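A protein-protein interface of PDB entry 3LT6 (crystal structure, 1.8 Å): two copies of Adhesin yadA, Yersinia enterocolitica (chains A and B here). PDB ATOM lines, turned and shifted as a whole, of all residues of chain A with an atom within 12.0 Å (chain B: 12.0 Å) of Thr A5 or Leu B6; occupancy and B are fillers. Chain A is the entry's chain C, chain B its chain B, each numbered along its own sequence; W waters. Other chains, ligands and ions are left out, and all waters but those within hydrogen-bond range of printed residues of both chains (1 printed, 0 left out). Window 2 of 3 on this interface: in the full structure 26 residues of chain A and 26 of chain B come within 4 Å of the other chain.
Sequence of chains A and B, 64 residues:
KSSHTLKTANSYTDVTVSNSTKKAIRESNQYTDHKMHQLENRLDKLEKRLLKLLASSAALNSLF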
ATOM      1  N   HIS A   4     -15.292  20.396 -33.495  1.00  0.00           N
ATOM      2  CA  HIS A   4     -15.435  20.771 -32.051  1.00  0.00           C
ATOM      3  C   HIS A   4     -15.881  19.551 -31.210  1.00  0.00           C
ATOM      4  O   HIS A   4     -15.202  19.151 -30.254  1.00  0.00           O
ATOM      5  CB  HIS A   4     -16.448  21.924 -31.872  1.00  0.00           C
ATOM      6  CG  HIS A   4     -16.068  23.221 -32.546  1.00  0.00           C
ATOM      7  ND1 HIS A   4     -16.839  23.807 -33.530  1.00  0.00           N
ATOM      8  CD2 HIS A   4     -15.030  24.072 -32.333  1.00  0.00           C
ATOM      9  CE1 HIS A   4     -16.288  24.948 -33.912  1.00  0.00           C
ATOM     10  NE2 HIS A   4     -15.183  25.130 -33.204  1.00  0.00           N
ATOM     11  N   THR A   5     -17.021  18.961 -31.567  1.00  0.00           N
ATOM     12  CA  THR A   5     -17.620  17.889 -30.762  1.00  0.00           C
ATOM     13  C   THR A   5     -16.867  16.555 -30.886  1.00  0.00           C
ATOM     14  O   THR A   5     -16.731  15.845 -29.888  1.00  0.00           O
ATOM     15  CB  THR A   5     -19.164  17.758 -31.007  1.00  0.00           C
ATOM     16  OG1 THR A   5     -19.822  18.928 -30.468  1.00  0.00           O
ATOM     17  CG2 THR A   5     -19.775  16.498 -30.368  1.00  0.00           C
ATOM     18  N   LEU A   6     -16.434  16.225 -32.104  1.00  0.00           N
ATOM     19  CA  LEU A   6     -15.629  15.036 -32.349  1.00  0.00           C
ATOM     20  C   LEU A   6     -14.325  15.058 -31.530  1.00  0.00           C
ATOM     21  O   LEU A   6     -14.048  14.096 -30.812  1.00  0.00           O
ATOM     22  CB  LEU A   6     -15.347  14.820 -33.834  1.00  0.00           C
ATOM     23  CG  LEU A   6     -15.322  13.383 -34.373  1.00  0.00           C
ATOM     24  CD1 LEU A   6     -14.201  13.224 -35.429  1.00  0.00           C
ATOM     25  CD2 LEU A   6     -15.222  12.293 -33.276  1.00  0.00           C
ATOM     26  N   LYS A   7     -13.553  16.151 -31.621  1.00  0.00           N
ATOM     27  CA  LYS A   7     -12.331  16.312 -30.786  1.00  0.00           C
ATOM     28  C   LYS A   7     -12.583  16.266 -29.282  1.00  0.00           C
ATOM     29  O   LYS A   7     -11.797  15.640 -28.561  1.00  0.00           O
ATOM     30  CB  LYS A   7     -11.552  17.590 -31.137  1.00  0.00           C
ATOM     31  CG  LYS A   7     -10.171  17.722 -30.477  1.00  0.00           C
ATOM     32  CD  LYS A   7      -9.387  18.907 -31.057  1.00  0.00           C
ATOM     33  CE  LYS A   7      -8.030  19.135 -30.422  1.00  0.00           C
ATOM     34  NZ  LYS A   7      -7.041  18.011 -30.637  1.00  0.00           N
ATOM     35  N   THR A   8     -13.661  16.909 -28.801  1.00  0.00           N
ATOM     36  CA  THR A   8     -13.980  16.882 -27.349  1.00  0.00           C
ATOM     37  C   THR A   8     -14.335  15.481 -26.802  1.00  0.00           C
ATOM     38  O   THR A   8     -13.892  15.087 -25.718  1.00  0.00           O
ATOM     39  CB  THR A   8     -15.147  17.862 -27.017  1.00  0.00           C
ATOM     40  OG1 THR A   8     -14.710  19.199 -27.285  1.00  0.00           O
ATOM     41  CG2 THR A   8     -15.522  17.772 -25.503  1.00  0.00           C
ATOM     42  N   ALA A   9     -15.160  14.740 -27.550  1.00  0.00           N
ATOM     43  CA  ALA A   9     -15.480  13.349 -27.206  1.00  0.00           C
ATOM     44  C   ALA A   9     -14.249  12.483 -27.230  1.00  0.00           C
ATOM     45  O   ALA A   9     -14.034  11.711 -26.303  1.00  0.00           O
ATOM     46  CB  ALA A   9     -16.493  12.769 -28.169  1.00  0.00           C
ATOM     47  N   ASN A  10     -13.470  12.579 -28.307  1.00  0.00           N
ATOM     48  CA  ASN A  10     -12.290  11.742 -28.415  1.00  0.00           C
ATOM     49  C   ASN A  10     -11.269  12.015 -27.304  1.00  0.00           C
ATOM     50  O   ASN A  10     -10.742  11.077 -26.691  1.00  0.00           O
ATOM     51  CB  ASN A  10     -11.671  11.799 -29.810  1.00  0.00           C
ATOM     52  CG  ASN A  10     -12.534  11.112 -30.861  1.00  0.00           C
ATOM     53  OD1 ASN A  10     -13.662  10.693 -30.593  1.00  0.00           O
ATOM     54  ND2 ASN A  10     -11.980  10.954 -32.060  1.00  0.00           N
ATOM     55  N   SER A  11     -11.029  13.287 -26.993  1.00  0.00           N
ATOM     56  CA  SER A  11     -10.203  13.592 -25.804  1.00  0.00           C
ATOM     57  C   SER A  11     -10.790  13.117 -24.442  1.00  0.00           C
ATOM     58  O   SER A  11     -10.059  12.606 -23.623  1.00  0.00           O
ATOM     59  CB  SER A  11      -9.763  15.067 -25.782  1.00  0.00           C
ATOM     60  OG  SER A  11     -10.857  15.886 -26.088  1.00  0.00           O
ATOM     61  N   TYR A  12     -12.098  13.248 -24.220  1.00  0.00           N
ATOM     62  CA  TYR A  12     -12.716  12.674 -23.029  1.00  0.00           C
ATOM     63  C   TYR A  12     -12.488  11.139 -22.957  1.00  0.00           C
ATOM     64  O   TYR A  12     -12.172  10.603 -21.884  1.00  0.00           O
ATOM     65  CB  TYR A  12     -14.219  12.986 -22.988  1.00  0.00           C
ATOM     66  CG  TYR A  12     -14.920  12.443 -21.776  1.00  0.00           C
ATOM     67  CD1 TYR A  12     -14.872  13.113 -20.564  1.00  0.00           C
ATOM     68  CD2 TYR A  12     -15.631  11.240 -21.834  1.00  0.00           C
ATOM     69  CE1 TYR A  12     -15.523  12.623 -19.441  1.00  0.00           C
ATOM     70  CE2 TYR A  12     -16.257  10.728 -20.710  1.00  0.00           C
ATOM     71  CZ  TYR A  12     -16.215  11.432 -19.515  1.00  0.00           C
ATOM     72  OH  TYR A  12     -16.813  10.931 -18.368  1.00  0.00           O
ATOM     73  N   THR A  13     -12.688  10.456 -24.081  1.00  0.00           N
ATOM     74  CA  THR A  13     -12.306   9.027 -24.234  1.00  0.00           C
ATOM     75  C   THR A  13     -10.853   8.778 -23.833  1.00  0.00           C
ATOM     76  O   THR A  13     -10.604   7.948 -22.970  1.00  0.00           O
ATOM     77  CB  THR A  13     -12.552   8.557 -25.677  1.00  0.00           C
ATOM     78  OG1 THR A  13     -13.935   8.769 -25.974  1.00  0.00           O
ATOM     79  CG2 THR A  13     -12.187   7.097 -25.844  1.00  0.00           C
ATOM     80  N   ASP A  14      -9.897   9.477 -24.470  1.00  0.00           N
ATOM     81  CA  ASP A  14      -8.470   9.318 -24.131  1.00  0.00           C
ATOM     82  C   ASP A  14      -8.165   9.404 -22.614  1.00  0.00           C
ATOM     83  O   ASP A  14      -7.505   8.535 -22.109  1.00  0.00           O
ATOM     84  CB  ASP A  14      -7.539  10.241 -24.928  1.00  0.00           C
ATOM     85  CG  ASP A  14      -7.516   9.942 -26.413  1.00  0.00           C
ATOM     86  OD1 ASP A  14      -7.907   8.835 -26.840  1.00  0.00           O
ATOM     87  OD2 ASP A  14      -7.139  10.849 -27.169  1.00  0.00           O
ATOM     88  N   VAL A  15      -8.692  10.407 -21.928  1.00  0.00           N
ATOM     89  CA  VAL A  15      -8.346  10.684 -20.494  1.00  0.00           C
ATOM     90  C   VAL A  15      -9.024   9.636 -19.591  1.00  0.00           C
ATOM     91  O   VAL A  15      -8.406   9.140 -18.703  1.00  0.00           O
ATOM     92  CB  VAL A  15      -8.817  12.099 -20.025  1.00  0.00           C
ATOM     93  CG1 VAL A  15      -8.180  12.441 -18.685  1.00  0.00           C
ATOM     94  CG2 VAL A  15      -8.478  13.140 -21.024  1.00  0.00           C
ATOM     95  N   THR A  16     -10.306   9.340 -19.848  1.00  0.00           N
ATOM     96  CA  THR A  16     -11.007   8.297 -19.098  1.00  0.00           C
ATOM     97  C   THR A  16     -10.532   6.896 -19.302  1.00  0.00           C
ATOM     98  O   THR A  16     -10.381   6.120 -18.335  1.00  0.00           O
ATOM     99  CB  THR A  16     -12.577   8.381 -19.224  1.00  0.00           C
ATOM    100  OG1 THR A  16     -12.984   8.247 -20.584  1.00  0.00           O
ATOM    101  CG2 THR A  16     -13.077   9.721 -18.706  1.00  0.00           C
ATOM    102  N   HIS B   4     -27.715  16.556 -26.188  1.00  0.00           N
ATOM    103  CA  HIS B   4     -26.708  16.757 -27.229  1.00  0.00           C
ATOM    104  C   HIS B   4     -25.827  15.521 -27.537  1.00  0.00           C
ATOM    105  O   HIS B   4     -25.609  14.610 -26.698  1.00  0.00           O
ATOM    106  CB  HIS B   4     -25.867  18.020 -26.968  1.00  0.00           C
ATOM    107  CG  HIS B   4     -26.499  19.275 -27.490  1.00  0.00           C
ATOM    108  ND1 HIS B   4     -27.039  19.368 -28.758  1.00  0.00           N
ATOM    109  CD2 HIS B   4     -26.683  20.488 -26.916  1.00  0.00           C
ATOM    110  CE1 HIS B   4     -27.526  20.582 -28.943  1.00  0.00           C
ATOM    111  NE2 HIS B   4     -27.333  21.278 -27.837  1.00  0.00           N
ATOM    112  N   THR B   5     -25.364  15.531 -28.781  1.00  0.00           N
ATOM    113  CA  THR B   5     -24.424  14.574 -29.344  1.00  0.00           C
ATOM    114  C   THR B   5     -23.218  14.316 -28.403  1.00  0.00           C
ATOM    115  O   THR B   5     -22.789  13.174 -28.226  1.00  0.00           O
ATOM    116  CB  THR B   5     -23.885  15.127 -30.688  1.00  0.00           C
ATOM    117  OG1 THR B   5     -24.991  15.460 -31.536  1.00  0.00           O
ATOM    118  CG2 THR B   5     -22.958  14.112 -31.397  1.00  0.00           C
ATOM    119  N   LEU B   6     -22.674  15.375 -27.826  1.00  0.00           N
ATOM    120  CA  LEU B   6     -21.507  15.226 -26.946  1.00  0.00           C
ATOM    121  C   LEU B   6     -21.893  14.443 -25.710  1.00  0.00           C
ATOM    122  O   LEU B   6     -21.168  13.499 -25.301  1.00  0.00           O
ATOM    123  CB  LEU B   6     -20.932  16.597 -26.619  1.00  0.00           C
ATOM    124  CG  LEU B   6     -19.718  16.776 -25.709  1.00  0.00           C
ATOM    125  CD1 LEU B   6     -18.452  15.983 -26.148  1.00  0.00           C
ATOM    126  CD2 LEU B   6     -19.446  18.307 -25.637  1.00  0.00           C
ATOM    127  N   LYS B   7     -23.032  14.819 -25.100  1.00  0.00           N
ATOM    128  CA  LYS B   7     -23.532  14.158 -23.905  1.00  0.00           C
ATOM    129  C   LYS B   7     -23.740  12.641 -24.192  1.00  0.00           C
ATOM    130  O   LYS B   7     -23.372  11.771 -23.366  1.00  0.00           O
ATOM    131  CB  LYS B   7     -24.866  14.825 -23.466  1.00  0.00           C
ATOM    132  CG  LYS B   7     -25.159  14.687 -22.019  1.00  0.00           C
ATOM    133  CD  LYS B   7     -26.548  15.127 -21.653  1.00  0.00           C
ATOM    134  CE  LYS B   7     -26.813  15.034 -20.161  1.00  0.00           C
ATOM    135  NZ  LYS B   7     -26.965  13.620 -19.734  1.00  0.00           N
ATOM    136  N   THR B   8     -24.331  12.330 -25.344  1.00  0.00           N
ATOM    137  CA  THR B   8     -24.561  10.945 -25.736  1.00  0.00           C
ATOM    138  C   THR B   8     -23.237  10.205 -25.990  1.00  0.00           C
ATOM    139  O   THR B   8     -23.070   9.072 -25.580  1.00  0.00           O
ATOM    140  CB  THR B   8     -25.400  10.860 -26.995  1.00  0.00           C
ATOM    141  OG1 THR B   8     -26.582  11.612 -26.771  1.00  0.00           O
ATOM    142  CG2 THR B   8     -25.777   9.357 -27.319  1.00  0.00           C
ATOM    143  N   ALA B   9     -22.313  10.840 -26.714  1.00  0.00           N
ATOM    144  CA  ALA B   9     -21.001  10.219 -26.959  1.00  0.00           C
ATOM    145  C   ALA B   9     -20.269   9.931 -25.644  1.00  0.00           C
ATOM    146  O   ALA B   9     -19.685   8.838 -25.452  1.00  0.00           O
ATOM    147  CB  ALA B   9     -20.162  11.167 -27.843  1.00  0.00           C
ATOM    148  N   ASN B  10     -20.349  10.870 -24.704  1.00  0.00           N
ATOM    149  CA  ASN B  10     -19.551  10.740 -23.450  1.00  0.00           C
ATOM    150  C   ASN B  10     -20.124   9.665 -22.544  1.00  0.00           C
ATOM    151  O   ASN B  10     -19.373   8.995 -21.843  1.00  0.00           O
ATOM    152  CB  ASN B  10     -19.527  12.005 -22.636  1.00  0.00           C
ATOM    153  CG  ASN B  10     -18.785  13.117 -23.287  1.00  0.00           C
ATOM    154  OD1 ASN B  10     -18.925  14.275 -22.871  1.00  0.00           O
ATOM    155  ND2 ASN B  10     -17.980  12.800 -24.260  1.00  0.00           N
ATOM    156  N   SER B  11     -21.467   9.590 -22.525  1.00  0.00           N
ATOM    157  CA  SER B  11     -22.244   8.534 -21.797  1.00  0.00           C
ATOM    158  C   SER B  11     -21.942   7.119 -22.335  1.00  0.00           C
ATOM    159  O   SER B  11     -21.677   6.156 -21.561  1.00  0.00           O
ATOM    160  CB  SER B  11     -23.746   8.798 -21.921  1.00  0.00           C
ATOM    161  OG  SER B  11     -24.154   9.584 -20.829  1.00  0.00           O
ATOM    162  N   TYR B  12     -21.977   6.985 -23.657  1.00  0.00           N
ATOM    163  CA  TYR B  12     -21.423   5.773 -24.292  1.00  0.00           C
ATOM    164  C   TYR B  12     -19.987   5.489 -23.840  1.00  0.00           C
ATOM    165  O   TYR B  12     -19.653   4.344 -23.447  1.00  0.00           O
ATOM    166  CB  TYR B  12     -21.517   5.805 -25.819  1.00  0.00           C
ATOM    167  CG  TYR B  12     -21.097   4.518 -26.430  1.00  0.00           C
ATOM    168  CD1 TYR B  12     -22.007   3.456 -26.567  1.00  0.00           C
ATOM    169  CD2 TYR B  12     -19.816   4.358 -26.906  1.00  0.00           C
ATOM    170  CE1 TYR B  12     -21.635   2.252 -27.154  1.00  0.00           C
ATOM    171  CE2 TYR B  12     -19.418   3.146 -27.530  1.00  0.00           C
ATOM    172  CZ  TYR B  12     -20.345   2.101 -27.647  1.00  0.00           C
ATOM    173  OH  TYR B  12     -19.966   0.921 -28.212  1.00  0.00           O
ATOM    174  N   THR B  13     -19.108   6.473 -23.945  1.00  0.00           N
ATOM    175  CA  THR B  13     -17.736   6.256 -23.416  1.00  0.00           C
ATOM    176  C   THR B  13     -17.688   5.772 -21.948  1.00  0.00           C
ATOM    177  O   THR B  13     -16.846   4.864 -21.599  1.00  0.00           O
ATOM    178  CB  THR B  13     -16.887   7.541 -23.577  1.00  0.00           C
ATOM    179  OG1 THR B  13     -16.808   7.872 -24.954  1.00  0.00           O
ATOM    180  CG2 THR B  13     -15.467   7.432 -22.975  1.00  0.00           C
ATOM    181  N   ASP B  14     -18.538   6.327 -21.062  1.00  0.00           N
ATOM    182  CA  ASP B  14     -18.490   5.969 -19.625  1.00  0.00           C
ATOM    183  C   ASP B  14     -18.905   4.502 -19.383  1.00  0.00           C
ATOM    184  O   ASP B  14     -18.291   3.810 -18.579  1.00  0.00           O
ATOM    185  CB  ASP B  14     -19.443   6.843 -18.813  1.00  0.00           C
ATOM    186  CG  ASP B  14     -19.067   8.316 -18.847  1.00  0.00           C
ATOM    187  OD1 ASP B  14     -17.877   8.606 -18.941  1.00  0.00           O
ATOM    188  OD2 ASP B  14     -19.951   9.213 -18.772  1.00  0.00           O
ATOM    189  N   VAL B  15     -19.971   4.061 -20.057  1.00  0.00           N
ATOM    190  CA  VAL B  15     -20.458   2.680 -19.959  1.00  0.00           C
ATOM    191  C   VAL B  15     -19.433   1.728 -20.528  1.00  0.00           C
ATOM    192  O   VAL B  15     -19.129   0.723 -19.907  1.00  0.00           O
ATOM    193  CB  VAL B  15     -21.857   2.547 -20.669  1.00  0.00           C
ATOM    194  CG1 VAL B  15     -22.409   1.091 -20.664  1.00  0.00           C
ATOM    195  CG2 VAL B  15     -22.810   3.440 -19.985  1.00  0.00           C
ATOM    196  N   THR B  16     -18.892   2.052 -21.700  1.00  0.00           N
ATOM    197  CA  THR B  16     -17.872   1.222 -22.346  1.00  0.00           C
ATOM    198  C   THR B  16     -16.561   1.047 -21.506  1.00  0.00           C
ATOM    199  O   THR B  16     -16.007  -0.084 -21.370  1.00  0.00           O
ATOM    200  CB  THR B  16     -17.703   1.660 -23.848  1.00  0.00           C
ATOM    201  OG1 THR B  16     -19.020   1.796 -24.497  1.00  0.00           O
ATOM    202  CG2 THR B  16     -16.859   0.604 -24.648  1.00  0.00           C
HETATM  203  O   HOH W   1     -16.551  10.422 -25.265  1.00  0.00           O
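Of chain B, only Leu B6 comes within 4 Å of Thr A5. No residue of chain B comes within 4 Å of His A4. No residue of chain B comes within 4 Å of Leu A6. Thr A8 touches one residue of chain B. No residue of chain A comes within 4 Å of His B4. No residue of chain A comes within 4 Å of Thr B5. No residue of chain A comes within 4 Å of Lys B7. No residue of chain A comes within 4 Å of Thr B8. Printed residues of chain B within 4 Å of Thr A13: Thr B13 (3.2 Å). Of the printed residues of chain B, Ala A9 touches Leu B6 (3.8 Å) and Asn B10 (3.9 Å). Printed residues of chain B within 4 Å of Tyr A12: Asn B10 (3.7 Å), Thr B13 (3.98 Å) and Asp B14 (2.6 Å). The nearest printed residue of chain A that does not touch Thr B13 is Ala A9 (4.9 Å).
Among the printed residues, merely in contact across the chains: Thr A8 with Leu B6 (3.5 Å), Thr A16 with Thr B13 (3.5 Å), Tyr A12 with Asn B10 (3.7 Å), Ala A9 with Leu B6 (3.8 Å), Ala A9 with Asn B10 (3.9 Å), Thr A5 with Leu B6 (3.9 Å) and Tyr A12 with Thr B13 (3.98 Å).
The side-chain hydroxyl of Thr A13 is in hydrogen-bond range of the side-chain hydroxyl of Thr B13 (3.2 Å). The side-chain carboxylate (OD1) of Asp B14 sits at hydrogen-bond distance from the side-chain hydroxyl (OH) of Tyr A12 (2.6 Å).
Thr A5 touches Leu B6, but with the chains exchanged Leu A6 does not touch Thr B5 (6.9 Å). Ala A9 touches Leu B6, but with the chains exchanged Leu A6 does not touch Ala B9 (7.4 Å). Ala A9 touches Asn B10, but with the chains exchanged Asn A10 does not touch Ala B9 (6.9 Å). Tyr A12 touches Thr B13, but with the chains exchanged Thr A13 does not touch Tyr B12 (7.2 Å). Of the 9 pairs that touch across the chains among the printed residues, 1 has its exchanged pair printed and touching as well.
Water W1 lies within hydrogen-bond range of the side-chain hydroxyl (OG1) of Thr B13, the side-chain amide nitrogen (ND2) of Asn B10, the backbone carbonyl oxygen (O) of Ala A9 and the side-chain hydroxyl (OG1) of Thr A13.
The side-chain hydroxyl (OG) of Ser A11 is in hydrogen-bond range of the backbone carbonyl oxygen (O) of Thr A8 (3.2 Å). O of Ala B9 sits at hydrogen-bond distance from OG1 of Thr B13, 3.1 Å away. The side-chain amide oxygen (OD1) of Asn B10 sits close to the backbone carbonyl oxygen (O) of Leu B6 (3.4 Å). OG1 of Thr A8 lies within hydrogen-bond range of O of His A4 (3.0 Å). O of Tyr A12 is in hydrogen-bond range of OG1 of Thr A16. O of Ala A9 sits at hydrogen-bond distance from OG1 of Thr A13.
Printed residues of chain B that touch a printed residue of chain A: Leu B6, Asn B10, Thr B13 and Asp B14. Printed residues of chain A that touch a printed residue of chain B: Thr A5, Thr A8, Ala A9, Tyr A12, Thr A13 and Thr A16. Among the printed residues, no Asp or Glu carboxylate lies within 4 Å of a Lys or Arg side-chain nitrogen of the other chain.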
